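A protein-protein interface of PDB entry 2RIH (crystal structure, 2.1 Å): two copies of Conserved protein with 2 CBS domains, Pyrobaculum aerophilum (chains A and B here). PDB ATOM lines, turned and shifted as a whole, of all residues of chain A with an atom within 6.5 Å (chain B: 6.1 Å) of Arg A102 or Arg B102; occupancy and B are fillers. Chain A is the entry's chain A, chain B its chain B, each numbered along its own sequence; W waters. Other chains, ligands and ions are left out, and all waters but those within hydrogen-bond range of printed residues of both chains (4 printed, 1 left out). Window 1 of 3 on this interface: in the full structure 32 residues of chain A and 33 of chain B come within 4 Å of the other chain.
Water W4 lies within hydrogen-bond range of the side-chain carboxylate (OE1) of Glu B56 (2.6 Å), the guanidinium group (NH1) of Arg A102 (3.1 Å) and the guanidinium group (NH2) of Arg B102 (3.3 Å).
Water W1 lies within hydrogen-bond range of the backbone carbonyl oxygen (O) of Ile A101 (2.8 Å), the guanidinium group (NH1) of Arg B120 (2.8 Å) and the backbone carbonyl oxygen (O) of Met A96 (3.2 Å).
Water W2 bridges NH1 of Arg B102 (2.8 Å) and NE2 of His A103 (3.5 Å).
Water W3 lies within hydrogen-bond range of the backbone carbonyl oxygen (O) of Glu B56 (2.8 Å) and the backbone carbonyl oxygen (O) of Glu A56 (2.9 Å).
Among the printed residues, pairs that only touch across the chains: Glu A56 with Glu B56, Ile A101 with Arg B120, Arg A102 with Arg B102, Ile A119 with Ile B119, Ile A119 with Arg B120, Phe A124 with Met B96, Phe A124 with Ile B101 and Phe A124 with Ile B119.
Glu A56 touches Arg B102, and with the chains exchanged Arg A102 touches Glu B56.
Arg A57 touches Arg B120, but with the chains exchanged Arg A120 does not touch Arg B57 (4.2 Å).
Arg A102 touches Arg B120, and with the chains exchanged Arg A120 touches Arg B102.
Ile A119 touches Arg B120, but with the chains exchanged Arg A120 does not touch Ile B119 (5.4 Å).
Positions printed for both chains: 37, 55, 56, 57, 96, 100, 101, 102, 103, 104, 117, 118, 119 and 120.
Of the 19 pairs that touch across the chains among the printed residues, 13 have their exchanged pair printed and touching as well.
Printed residues of chain B within 4 Å of Arg A102: Glu B56 (2.8 Å), Arg B102 (3.7 Å) and Arg B120 (3.2 Å).
Of the printed residues of chain B, Ile A119 touches Ile B119 (3.8 Å) and Arg B120 (3.8 Å).
Of the printed residues of chain B, Arg A120 touches Asn B100 (2.7 Å) and Arg B102 (3.1 Å).
Of the printed residues of chain A, Glu B56 touches Glu A56 (3.6 Å), Arg A57 (3.3 Å) and Arg A102 (2.8 Å).
Printed residues of chain A within 4 Å of Arg B57: Gly A37 and Glu A56.
Printed residues of chain A within 4 Å of Met B96: Phe A124.
Of the printed residues of chain A, Arg B102 touches Glu A56 (3.0 Å), Arg A102 (3.7 Å) and Arg A120 (3.1 Å).
The nearest printed residue of chain B that does not touch Glu A56 is Ser B55 (5.4 Å).
The guanidinium group (NE) of Arg B57 is in salt-bridge range of the side-chain carboxylate (OE2) of Glu A56.
NH1 of Arg B102 is in salt-bridge range of OE1 of Glu A56, at 3.0 Å.
The guanidinium group (NE) of Arg A57 is in salt-bridge range of the side-chain carboxylate (OE2) of Glu B56 (3.3 Å).
The backbone carbonyl oxygen (O) of Asn A100 lies within hydrogen-bond range of the guanidinium group (NH1) of Arg B120, 3.2 Å away.
The side-chain carboxylate (OE1) of Glu B56 is in salt-bridge range of the guanidinium group (NH2) of Arg A102, 2.8 Å away.
The backbone carbonyl oxygen (O) of Asn B100 sits at hydrogen-bond distance from the guanidinium group (NH2) of Arg A120 (2.7 Å).
The backbone NH of Gly A37 lies close to the guanidinium group of Arg B57 (3.3 Å).
The backbone NH (N) of Gly B37 sits close to the guanidinium group (NH2) of Arg A57, at 3.2 Å.
The guanidinium group (NH2) of Arg B120 sits close to the guanidinium group (NH1) of Arg A57.
NE of Arg A102 lies close to NH2 of Arg B120 (3.4 Å).
The guanidinium group (NH1) of Arg A120 sits close to the guanidinium group (NE) of Arg B102 (3.1 Å).
The backbone carbonyl oxygen of Arg A102 sits at hydrogen-bond distance from the backbone NH of Ile A119, 3.0 Å away.
The backbone NH (N) of Arg A120 is in hydrogen-bond range of the side-chain hydroxyl (OG) of Ser A118, at 3.0 Å.
The backbone carbonyl oxygen (O) of Gly B37 lies within hydrogen-bond range of the backbone NH (N) of Glu B56 (2.9 Å).
The backbone NH of Ile B101 is in hydrogen-bond range of the backbone carbonyl oxygen of Met B96, at 2.8 Å.
SD of Met B96 lies within hydrogen-bond range of N of Ile B119 (3.7 Å).
The side-chain hydroxyl (OG) of Ser B118 is in hydrogen-bond range of the backbone NH (N) of Arg B120 (3.0 Å).
Printed residues of chain A that touch a printed residue of chain B: Gly A37, Glu A56, Arg A57, Asn A100, Ile A101, Arg A102, Ile A119, Arg A120 and Phe A124.
Along chain A the printed residues that touch a printed residue of chain B span positions 37 to 124.
Hydrophobic or aromatic side chains of chain B that line the printed part of chain A: Met B96 and Ile B119.
Among the printed residues, Asp or Glu carboxylates within 4 Å of a Lys or Arg side-chain nitrogen of the other chain: Glu A56 with Arg B57 (2.8 Å), Glu A56 with Arg B102 (3.0 Å), Arg A57 with Glu B56 (3.3 Å) and Arg A102 with Glu B56 (2.8 Å).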
ATOM      1  N   GLY A  37      33.220 -11.197   2.392  1.00  0.00           N
ATOM      2  CA  GLY A  37      32.544 -12.460   2.110  1.00  0.00           C
ATOM      3  C   GLY A  37      31.357 -12.430   1.179  1.00  0.00           C
ATOM      4  O   GLY A  37      30.798 -13.486   0.883  1.00  0.00           O
ATOM      5  N   SER A  55      28.046 -15.188  -2.069  1.00  0.00           N
ATOM      6  CA  SER A  55      28.900 -15.160  -0.893  1.00  0.00           C
ATOM      7  C   SER A  55      29.850 -16.347  -0.892  1.00  0.00           C
ATOM      8  O   SER A  55      29.698 -17.292  -1.673  1.00  0.00           O
ATOM      9  CB  SER A  55      28.068 -15.158   0.382  1.00  0.00           C
ATOM     10  OG  SER A  55      27.345 -16.359   0.496  1.00  0.00           O
ATOM     11  N   GLU A  56      30.842 -16.269  -0.016  1.00  0.00           N
ATOM     12  CA  GLU A  56      31.767 -17.363   0.237  1.00  0.00           C
ATOM     13  C   GLU A  56      31.028 -18.654   0.597  1.00  0.00           C
ATOM     14  O   GLU A  56      31.526 -19.755   0.348  1.00  0.00           O
ATOM     15  CB  GLU A  56      32.741 -16.972   1.353  1.00  0.00           C
ATOM     16  CG  GLU A  56      32.095 -16.652   2.678  1.00  0.00           C
ATOM     17  CD  GLU A  56      33.054 -16.000   3.651  1.00  0.00           C
ATOM     18  OE1 GLU A  56      32.601 -15.159   4.441  1.00  0.00           O
ATOM     19  OE2 GLU A  56      34.254 -16.316   3.625  1.00  0.00           O
ATOM     20  N   ARG A  57      29.843 -18.513   1.185  1.00  0.00           N
ATOM     21  CA  ARG A  57      28.997 -19.657   1.469  1.00  0.00           C
ATOM     22  C   ARG A  57      28.478 -20.350   0.210  1.00  0.00           C
ATOM     23  O   ARG A  57      28.369 -21.579   0.172  1.00  0.00           O
ATOM     24  CB  ARG A  57      27.825 -19.255   2.354  1.00  0.00           C
ATOM     25  CG  ARG A  57      26.989 -20.458   2.729  1.00  0.00           C
ATOM     26  CD  ARG A  57      26.450 -20.370   4.127  1.00  0.00           C
ATOM     27  NE  ARG A  57      27.527 -20.295   5.109  1.00  0.00           N
ATOM     28  CZ  ARG A  57      27.329 -20.322   6.420  1.00  0.00           C
ATOM     29  NH1 ARG A  57      26.103 -20.456   6.911  1.00  0.00           N
ATOM     30  NH2 ARG A  57      28.362 -20.221   7.236  1.00  0.00           N
ATOM     31  N   MET A  96      18.970  -9.781   8.385  1.00  0.00           N
ATOM     32  CA  MET A  96      19.946 -10.862   8.492  1.00  0.00           C
ATOM     33  C   MET A  96      19.356 -12.038   9.258  1.00  0.00           C
ATOM     34  O   MET A  96      19.476 -13.180   8.825  1.00  0.00           O
ATOM     35  CB  MET A  96      21.227 -10.398   9.185  1.00  0.00           C
ATOM     36  CG  MET A  96      22.102  -9.548   8.325  1.00  0.00           C
ATOM     37  SD  MET A  96      23.561  -9.017   9.211  1.00  0.00           S
ATOM     38  CE  MET A  96      23.990  -7.605   8.200  1.00  0.00           C
ATOM     39  N   ASN A 100      18.255 -15.559   7.469  1.00  0.00           N
ATOM     40  CA  ASN A 100      19.337 -16.501   7.799  1.00  0.00           C
ATOM     41  C   ASN A 100      20.612 -16.233   7.002  1.00  0.00           C
ATOM     42  O   ASN A 100      21.259 -17.162   6.505  1.00  0.00           O
ATOM     43  CB  ASN A 100      18.873 -17.958   7.613  1.00  0.00           C
ATOM     44  CG  ASN A 100      17.698 -18.316   8.500  1.00  0.00           C
ATOM     45  OD1 ASN A 100      17.596 -17.837   9.626  1.00  0.00           O
ATOM     46  ND2 ASN A 100      16.813 -19.175   8.003  1.00  0.00           N
ATOM     47  N   ILE A 101      20.961 -14.949   6.897  1.00  0.00           N
ATOM     48  CA  ILE A 101      22.139 -14.499   6.166  1.00  0.00           C
ATOM     49  C   ILE A 101      23.016 -13.649   7.080  1.00  0.00           C
ATOM     50  O   ILE A 101      22.616 -13.278   8.199  1.00  0.00           O
ATOM     51  CB  ILE A 101      21.780 -13.710   4.862  1.00  0.00           C
ATOM     52  CG1 ILE A 101      20.896 -12.490   5.151  1.00  0.00           C
ATOM     53  CG2 ILE A 101      21.110 -14.636   3.837  1.00  0.00           C
ATOM     54  CD1 ILE A 101      20.353 -11.798   3.883  1.00  0.00           C
ATOM     55  N   ARG A 102      24.228 -13.376   6.623  1.00  0.00           N
ATOM     56  CA  ARG A 102      25.181 -12.636   7.431  1.00  0.00           C
ATOM     57  C   ARG A 102      25.638 -11.360   6.757  1.00  0.00           C
ATOM     58  O   ARG A 102      26.575 -10.716   7.218  1.00  0.00           O
ATOM     59  CB  ARG A 102      26.361 -13.531   7.779  1.00  0.00           C
ATOM     60  CG  ARG A 102      25.982 -14.653   8.719  1.00  0.00           C
ATOM     61  CD  ARG A 102      27.120 -15.633   8.860  1.00  0.00           C
ATOM     62  NE  ARG A 102      27.512 -16.110   7.541  1.00  0.00           N
ATOM     63  CZ  ARG A 102      28.696 -16.632   7.246  1.00  0.00           C
ATOM     64  NH1 ARG A 102      29.618 -16.795   8.187  1.00  0.00           N
ATOM     65  NH2 ARG A 102      28.946 -17.001   5.997  1.00  0.00           N
ATOM     66  N   HIS A 103      24.963 -11.003   5.670  1.00  0.00           N
ATOM     67  CA  HIS A 103      25.226  -9.774   4.928  1.00  0.00           C
ATOM     68  C   HIS A 103      23.913  -9.206   4.432  1.00  0.00           C
ATOM     69  O   HIS A 103      22.926  -9.929   4.329  1.00  0.00           O
ATOM     70  CB  HIS A 103      26.110 -10.049   3.701  1.00  0.00           C
ATOM     71  CG  HIS A 103      27.485 -10.530   4.041  1.00  0.00           C
ATOM     72  ND1 HIS A 103      27.774 -11.862   4.246  1.00  0.00           N
ATOM     73  CD2 HIS A 103      28.650  -9.861   4.208  1.00  0.00           C
ATOM     74  CE1 HIS A 103      29.059 -11.989   4.526  1.00  0.00           C
ATOM     75  NE2 HIS A 103      29.611 -10.792   4.517  1.00  0.00           N
ATOM     76  N   VAL A 104      23.911  -7.904   4.149  1.00  0.00           N
ATOM     77  CA  VAL A 104      22.846  -7.259   3.392  1.00  0.00           C
ATOM     78  C   VAL A 104      23.482  -6.269   2.430  1.00  0.00           C
ATOM     79  O   VAL A 104      24.529  -5.665   2.722  1.00  0.00           O
ATOM     80  CB  VAL A 104      21.781  -6.517   4.262  1.00  0.00           C
ATOM     81  CG1 VAL A 104      20.928  -7.504   5.025  1.00  0.00           C
ATOM     82  CG2 VAL A 104      22.430  -5.496   5.193  1.00  0.00           C
ATOM     83  N   LEU A 117      26.860  -4.491   4.049  1.00  0.00           N
ATOM     84  CA  LEU A 117      26.983  -4.500   5.491  1.00  0.00           C
ATOM     85  C   LEU A 117      27.077  -5.954   5.956  1.00  0.00           C
ATOM     86  O   LEU A 117      26.314  -6.809   5.511  1.00  0.00           O
ATOM     87  CB  LEU A 117      25.758  -3.815   6.100  1.00  0.00           C
ATOM     88  CG  LEU A 117      25.769  -3.461   7.584  1.00  0.00           C
ATOM     89  CD1 LEU A 117      26.711  -2.284   7.852  1.00  0.00           C
ATOM     90  CD2 LEU A 117      24.349  -3.135   8.058  1.00  0.00           C
ATOM     91  N   SER A 118      28.030  -6.217   6.843  1.00  0.00           N
ATOM     92  CA  SER A 118      28.242  -7.529   7.397  1.00  0.00           C
ATOM     93  C   SER A 118      27.739  -7.606   8.837  1.00  0.00           C
ATOM     94  O   SER A 118      27.587  -6.593   9.511  1.00  0.00           O
ATOM     95  CB  SER A 118      29.735  -7.846   7.385  1.00  0.00           C
ATOM     96  OG  SER A 118      29.990  -9.015   8.113  1.00  0.00           O
ATOM     97  N   ILE A 119      27.513  -8.831   9.297  1.00  0.00           N
ATOM     98  CA  ILE A 119      27.220  -9.100  10.694  1.00  0.00           C
ATOM     99  C   ILE A 119      28.394  -8.647  11.607  1.00  0.00           C
ATOM    100  O   ILE A 119      28.187  -8.241  12.753  1.00  0.00           O
ATOM    101  CB  ILE A 119      26.875 -10.597  10.883  1.00  0.00           C
ATOM    102  CG1 ILE A 119      26.191 -10.831  12.227  1.00  0.00           C
ATOM    103  CG2 ILE A 119      28.125 -11.485  10.732  1.00  0.00           C
ATOM    104  CD1 ILE A 119      25.464 -12.160  12.284  1.00  0.00           C
ATOM    105  N   ARG A 120      29.615  -8.681  11.081  1.00  0.00           N
ATOM    106  CA  ARG A 120      30.794  -8.119  11.776  1.00  0.00           C
ATOM    107  C   ARG A 120      30.641  -6.649  12.114  1.00  0.00           C
ATOM    108  O   ARG A 120      31.108  -6.196  13.167  1.00  0.00           O
ATOM    109  CB  ARG A 120      32.025  -8.192  10.888  1.00  0.00           C
ATOM    110  CG  ARG A 120      32.843  -9.420  10.977  1.00  0.00           C
ATOM    111  CD  ARG A 120      33.841  -9.396   9.823  1.00  0.00           C
ATOM    112  NE  ARG A 120      35.093  -9.991  10.218  1.00  0.00           N
ATOM    113  CZ  ARG A 120      35.635 -11.091   9.723  1.00  0.00           C
ATOM    114  NH1 ARG A 120      35.081 -11.788   8.737  1.00  0.00           N
ATOM    115  NH2 ARG A 120      36.780 -11.475  10.239  1.00  0.00           N
ATOM    116  N   PHE A 124      29.884  -6.132  16.996  1.00  0.00           N
ATOM    117  CA  PHE A 124      31.047  -5.950  17.873  1.00  0.00           C
ATOM    118  C   PHE A 124      30.943  -4.741  18.826  1.00  0.00           C
ATOM    119  O   PHE A 124      31.157  -4.880  20.036  1.00  0.00           O
ATOM    120  CB  PHE A 124      32.332  -5.860  17.041  1.00  0.00           C
ATOM    121  CG  PHE A 124      32.764  -7.170  16.401  1.00  0.00           C
ATOM    122  CD1 PHE A 124      32.356  -8.406  16.900  1.00  0.00           C
ATOM    123  CD2 PHE A 124      33.644  -7.154  15.326  1.00  0.00           C
ATOM    124  CE1 PHE A 124      32.782  -9.596  16.305  1.00  0.00           C
ATOM    125  CE2 PHE A 124      34.088  -8.340  14.734  1.00  0.00           C
ATOM    126  CZ  PHE A 124      33.647  -9.562  15.225  1.00  0.00           C
ATOM    127  N   GLY B  37      30.125 -21.961   9.246  1.00  0.00           N
ATOM    128  CA  GLY B  37      31.279 -21.384   8.583  1.00  0.00           C
ATOM    129  C   GLY B  37      32.664 -21.835   9.014  1.00  0.00           C
ATOM    130  O   GLY B  37      33.621 -21.562   8.306  1.00  0.00           O
ATOM    131  N   SER B  55      38.059 -22.275   7.902  1.00  0.00           N
ATOM    132  CA  SER B  55      36.927 -21.415   7.660  1.00  0.00           C
ATOM    133  C   SER B  55      36.531 -21.509   6.203  1.00  0.00           C
ATOM    134  O   SER B  55      37.350 -21.830   5.351  1.00  0.00           O
ATOM    135  CB  SER B  55      37.325 -19.964   7.963  1.00  0.00           C
ATOM    136  OG  SER B  55      36.224 -19.097   7.782  1.00  0.00           O
ATOM    137  N   GLU B  56      35.273 -21.201   5.922  1.00  0.00           N
ATOM    138  CA  GLU B  56      34.822 -21.004   4.538  1.00  0.00           C
ATOM    139  C   GLU B  56      35.661 -19.924   3.824  1.00  0.00           C
ATOM    140  O   GLU B  56      35.835 -19.969   2.604  1.00  0.00           O
ATOM    141  CB  GLU B  56      33.334 -20.640   4.513  1.00  0.00           C
ATOM    142  CG  GLU B  56      33.018 -19.308   5.100  1.00  0.00           C
ATOM    143  CD  GLU B  56      31.548 -19.149   5.412  1.00  0.00           C
ATOM    144  OE1 GLU B  56      31.250 -18.539   6.450  1.00  0.00           O
ATOM    145  OE2 GLU B  56      30.706 -19.645   4.637  1.00  0.00           O
ATOM    146  N   ARG B  57      36.195 -18.981   4.600  1.00  0.00           N
ATOM    147  CA  ARG B  57      37.123 -17.966   4.098  1.00  0.00           C
ATOM    148  C   ARG B  57      38.420 -18.570   3.533  1.00  0.00           C
ATOM    149  O   ARG B  57      38.933 -18.113   2.511  1.00  0.00           O
ATOM    150  CB  ARG B  57      37.443 -16.970   5.230  1.00  0.00           C
ATOM    151  CG  ARG B  57      38.305 -15.763   4.841  1.00  0.00           C
ATOM    152  CD  ARG B  57      37.704 -14.955   3.688  1.00  0.00           C
ATOM    153  NE  ARG B  57      36.345 -14.485   3.964  1.00  0.00           N
ATOM    154  CZ  ARG B  57      36.031 -13.311   4.519  1.00  0.00           C
ATOM    155  NH1 ARG B  57      36.955 -12.419   4.858  1.00  0.00           N
ATOM    156  NH2 ARG B  57      34.761 -13.020   4.724  1.00  0.00           N
ATOM    157  N   MET B  96      36.312 -12.688  19.573  1.00  0.00           N
ATOM    158  CA  MET B  96      35.872 -12.510  18.182  1.00  0.00           C
ATOM    159  C   MET B  96      36.206 -11.104  17.666  1.00  0.00           C
ATOM    160  O   MET B  96      36.719 -10.926  16.565  1.00  0.00           O
ATOM    161  CB  MET B  96      34.360 -12.729  18.079  1.00  0.00           C
ATOM    162  CG  MET B  96      33.920 -14.190  18.214  1.00  0.00           C
ATOM    163  SD  MET B  96      32.144 -14.356  17.969  1.00  0.00           S
ATOM    164  CE  MET B  96      31.813 -15.956  18.707  1.00  0.00           C
ATOM    165  N   ASN B 100      39.281 -10.246  15.400  1.00  0.00           N
ATOM    166  CA  ASN B 100      38.543 -10.037  14.147  1.00  0.00           C
ATOM    167  C   ASN B 100      38.158 -11.348  13.468  1.00  0.00           C
ATOM    168  O   ASN B 100      38.496 -11.587  12.305  1.00  0.00           O
ATOM    169  CB  ASN B 100      39.339  -9.153  13.180  1.00  0.00           C
ATOM    170  CG  ASN B 100      38.525  -8.729  11.966  1.00  0.00           C
ATOM    171  OD1 ASN B 100      37.312  -8.478  12.065  1.00  0.00           O
ATOM    172  ND2 ASN B 100      39.186  -8.642  10.813  1.00  0.00           N
ATOM    173  N   ILE B 101      37.476 -12.206  14.217  1.00  0.00           N
ATOM    174  CA  ILE B 101      37.008 -13.482  13.699  1.00  0.00           C
ATOM    175  C   ILE B 101      35.540 -13.645  14.046  1.00  0.00           C
ATOM    176  O   ILE B 101      35.044 -13.018  14.988  1.00  0.00           O
ATOM    177  CB  ILE B 101      37.849 -14.684  14.218  1.00  0.00           C
ATOM    178  CG1 ILE B 101      37.900 -14.699  15.754  1.00  0.00           C
ATOM    179  CG2 ILE B 101      39.250 -14.644  13.598  1.00  0.00           C
ATOM    180  CD1 ILE B 101      38.704 -15.845  16.352  1.00  0.00           C
ATOM    181  N   ARG B 102      34.845 -14.479  13.282  1.00  0.00           N
ATOM    182  CA  ARG B 102      33.404 -14.635  13.454  1.00  0.00           C
ATOM    183  C   ARG B 102      33.023 -15.880  14.230  1.00  0.00           C
ATOM    184  O   ARG B 102      31.844 -16.180  14.354  1.00  0.00           O
ATOM    185  CB  ARG B 102      32.708 -14.618  12.094  1.00  0.00           C
ATOM    186  CG  ARG B 102      32.845 -13.290  11.376  1.00  0.00           C
ATOM    187  CD  ARG B 102      32.397 -13.403   9.942  1.00  0.00           C
ATOM    188  NE  ARG B 102      33.265 -14.305   9.197  1.00  0.00           N
ATOM    189  CZ  ARG B 102      33.083 -14.649   7.926  1.00  0.00           C
ATOM    190  NH1 ARG B 102      32.060 -14.154   7.236  1.00  0.00           N
ATOM    191  NH2 ARG B 102      33.937 -15.480   7.339  1.00  0.00           N
ATOM    192  N   HIS B 103      34.021 -16.602  14.738  1.00  0.00           N
ATOM    193  CA  HIS B 103      33.792 -17.803  15.551  1.00  0.00           C
ATOM    194  C   HIS B 103      34.819 -17.906  16.655  1.00  0.00           C
ATOM    195  O   HIS B 103      35.900 -17.326  16.563  1.00  0.00           O
ATOM    196  CB  HIS B 103      33.915 -19.080  14.703  1.00  0.00           C
ATOM    197  CG  HIS B 103      32.904 -19.186  13.610  1.00  0.00           C
ATOM    198  ND1 HIS B 103      33.102 -18.645  12.356  1.00  0.00           N
ATOM    199  CD2 HIS B 103      31.690 -19.784  13.576  1.00  0.00           C
ATOM    200  CE1 HIS B 103      32.038 -18.883  11.607  1.00  0.00           C
ATOM    201  NE2 HIS B 103      31.174 -19.581  12.320  1.00  0.00           N
ATOM    202  N   VAL B 104      34.471 -18.648  17.698  1.00  0.00           N
ATOM    203  CA  VAL B 104      35.442 -19.114  18.673  1.00  0.00           C
ATOM    204  C   VAL B 104      35.187 -20.595  18.903  1.00  0.00           C
ATOM    205  O   VAL B 104      34.046 -21.062  18.787  1.00  0.00           O
ATOM    206  CB  VAL B 104      35.406 -18.314  20.007  1.00  0.00           C
ATOM    207  CG1 VAL B 104      36.120 -16.969  19.836  1.00  0.00           C
ATOM    208  CG2 VAL B 104      33.975 -18.124  20.502  1.00  0.00           C
ATOM    209  N   LEU B 117      31.155 -21.485  18.686  1.00  0.00           N
ATOM    210  CA  LEU B 117      30.226 -20.385  18.821  1.00  0.00           C
ATOM    211  C   LEU B 117      30.424 -19.399  17.669  1.00  0.00           C
ATOM    212  O   LEU B 117      31.544 -19.030  17.351  1.00  0.00           O
ATOM    213  CB  LEU B 117      30.448 -19.694  20.177  1.00  0.00           C
ATOM    214  CG  LEU B 117      29.222 -19.099  20.870  1.00  0.00           C
ATOM    215  CD1 LEU B 117      28.118 -20.140  21.061  1.00  0.00           C
ATOM    216  CD2 LEU B 117      29.625 -18.497  22.215  1.00  0.00           C
ATOM    217  N   SER B 118      29.316 -18.977  17.065  1.00  0.00           N
ATOM    218  CA  SER B 118      29.305 -17.985  15.992  1.00  0.00           C
ATOM    219  C   SER B 118      28.873 -16.614  16.515  1.00  0.00           C
ATOM    220  O   SER B 118      28.081 -16.532  17.446  1.00  0.00           O
ATOM    221  CB  SER B 118      28.307 -18.411  14.915  1.00  0.00           C
ATOM    222  OG  SER B 118      28.177 -17.411  13.934  1.00  0.00           O
ATOM    223  N   ILE B 119      29.359 -15.546  15.885  1.00  0.00           N
ATOM    224  CA  ILE B 119      28.882 -14.185  16.191  1.00  0.00           C
ATOM    225  C   ILE B 119      27.364 -14.099  15.969  1.00  0.00           C
ATOM    226  O   ILE B 119      26.656 -13.366  16.672  1.00  0.00           O
ATOM    227  CB  ILE B 119      29.645 -13.105  15.370  1.00  0.00           C
ATOM    228  CG1 ILE B 119      29.275 -11.685  15.835  1.00  0.00           C
ATOM    229  CG2 ILE B 119      29.396 -13.278  13.867  1.00  0.00           C
ATOM    230  CD1 ILE B 119      29.567 -11.397  17.308  1.00  0.00           C
ATOM    231  N   ARG B 120      26.885 -14.890  15.011  1.00  0.00           N
ATOM    232  CA  ARG B 120      25.464 -15.064  14.732  1.00  0.00           C
ATOM    233  C   ARG B 120      24.697 -15.591  15.968  1.00  0.00           C
ATOM    234  O   ARG B 120      23.549 -15.212  16.192  1.00  0.00           O
ATOM    235  CB  ARG B 120      25.302 -16.024  13.536  1.00  0.00           C
ATOM    236  CG  ARG B 120      24.038 -15.842  12.726  1.00  0.00           C
ATOM    237  CD  ARG B 120      23.602 -17.142  12.043  1.00  0.00           C
ATOM    238  NE  ARG B 120      24.485 -17.573  10.952  1.00  0.00           N
ATOM    239  CZ  ARG B 120      24.159 -17.581   9.656  1.00  0.00           C
ATOM    240  NH1 ARG B 120      22.967 -17.169   9.242  1.00  0.00           N
ATOM    241  NH2 ARG B 120      25.028 -18.008   8.751  1.00  0.00           N
HETATM  242  O   HOH W   1      21.805 -14.873  10.290  1.00  0.00           O
HETATM  243  O   HOH W   2      29.765 -12.521   7.537  1.00  0.00           O
HETATM  244  O   HOH W   3      34.216 -20.700   0.378  1.00  0.00           O
HETATM  245  O   HOH W   4      32.455 -18.073   8.669  1.00  0.00           O
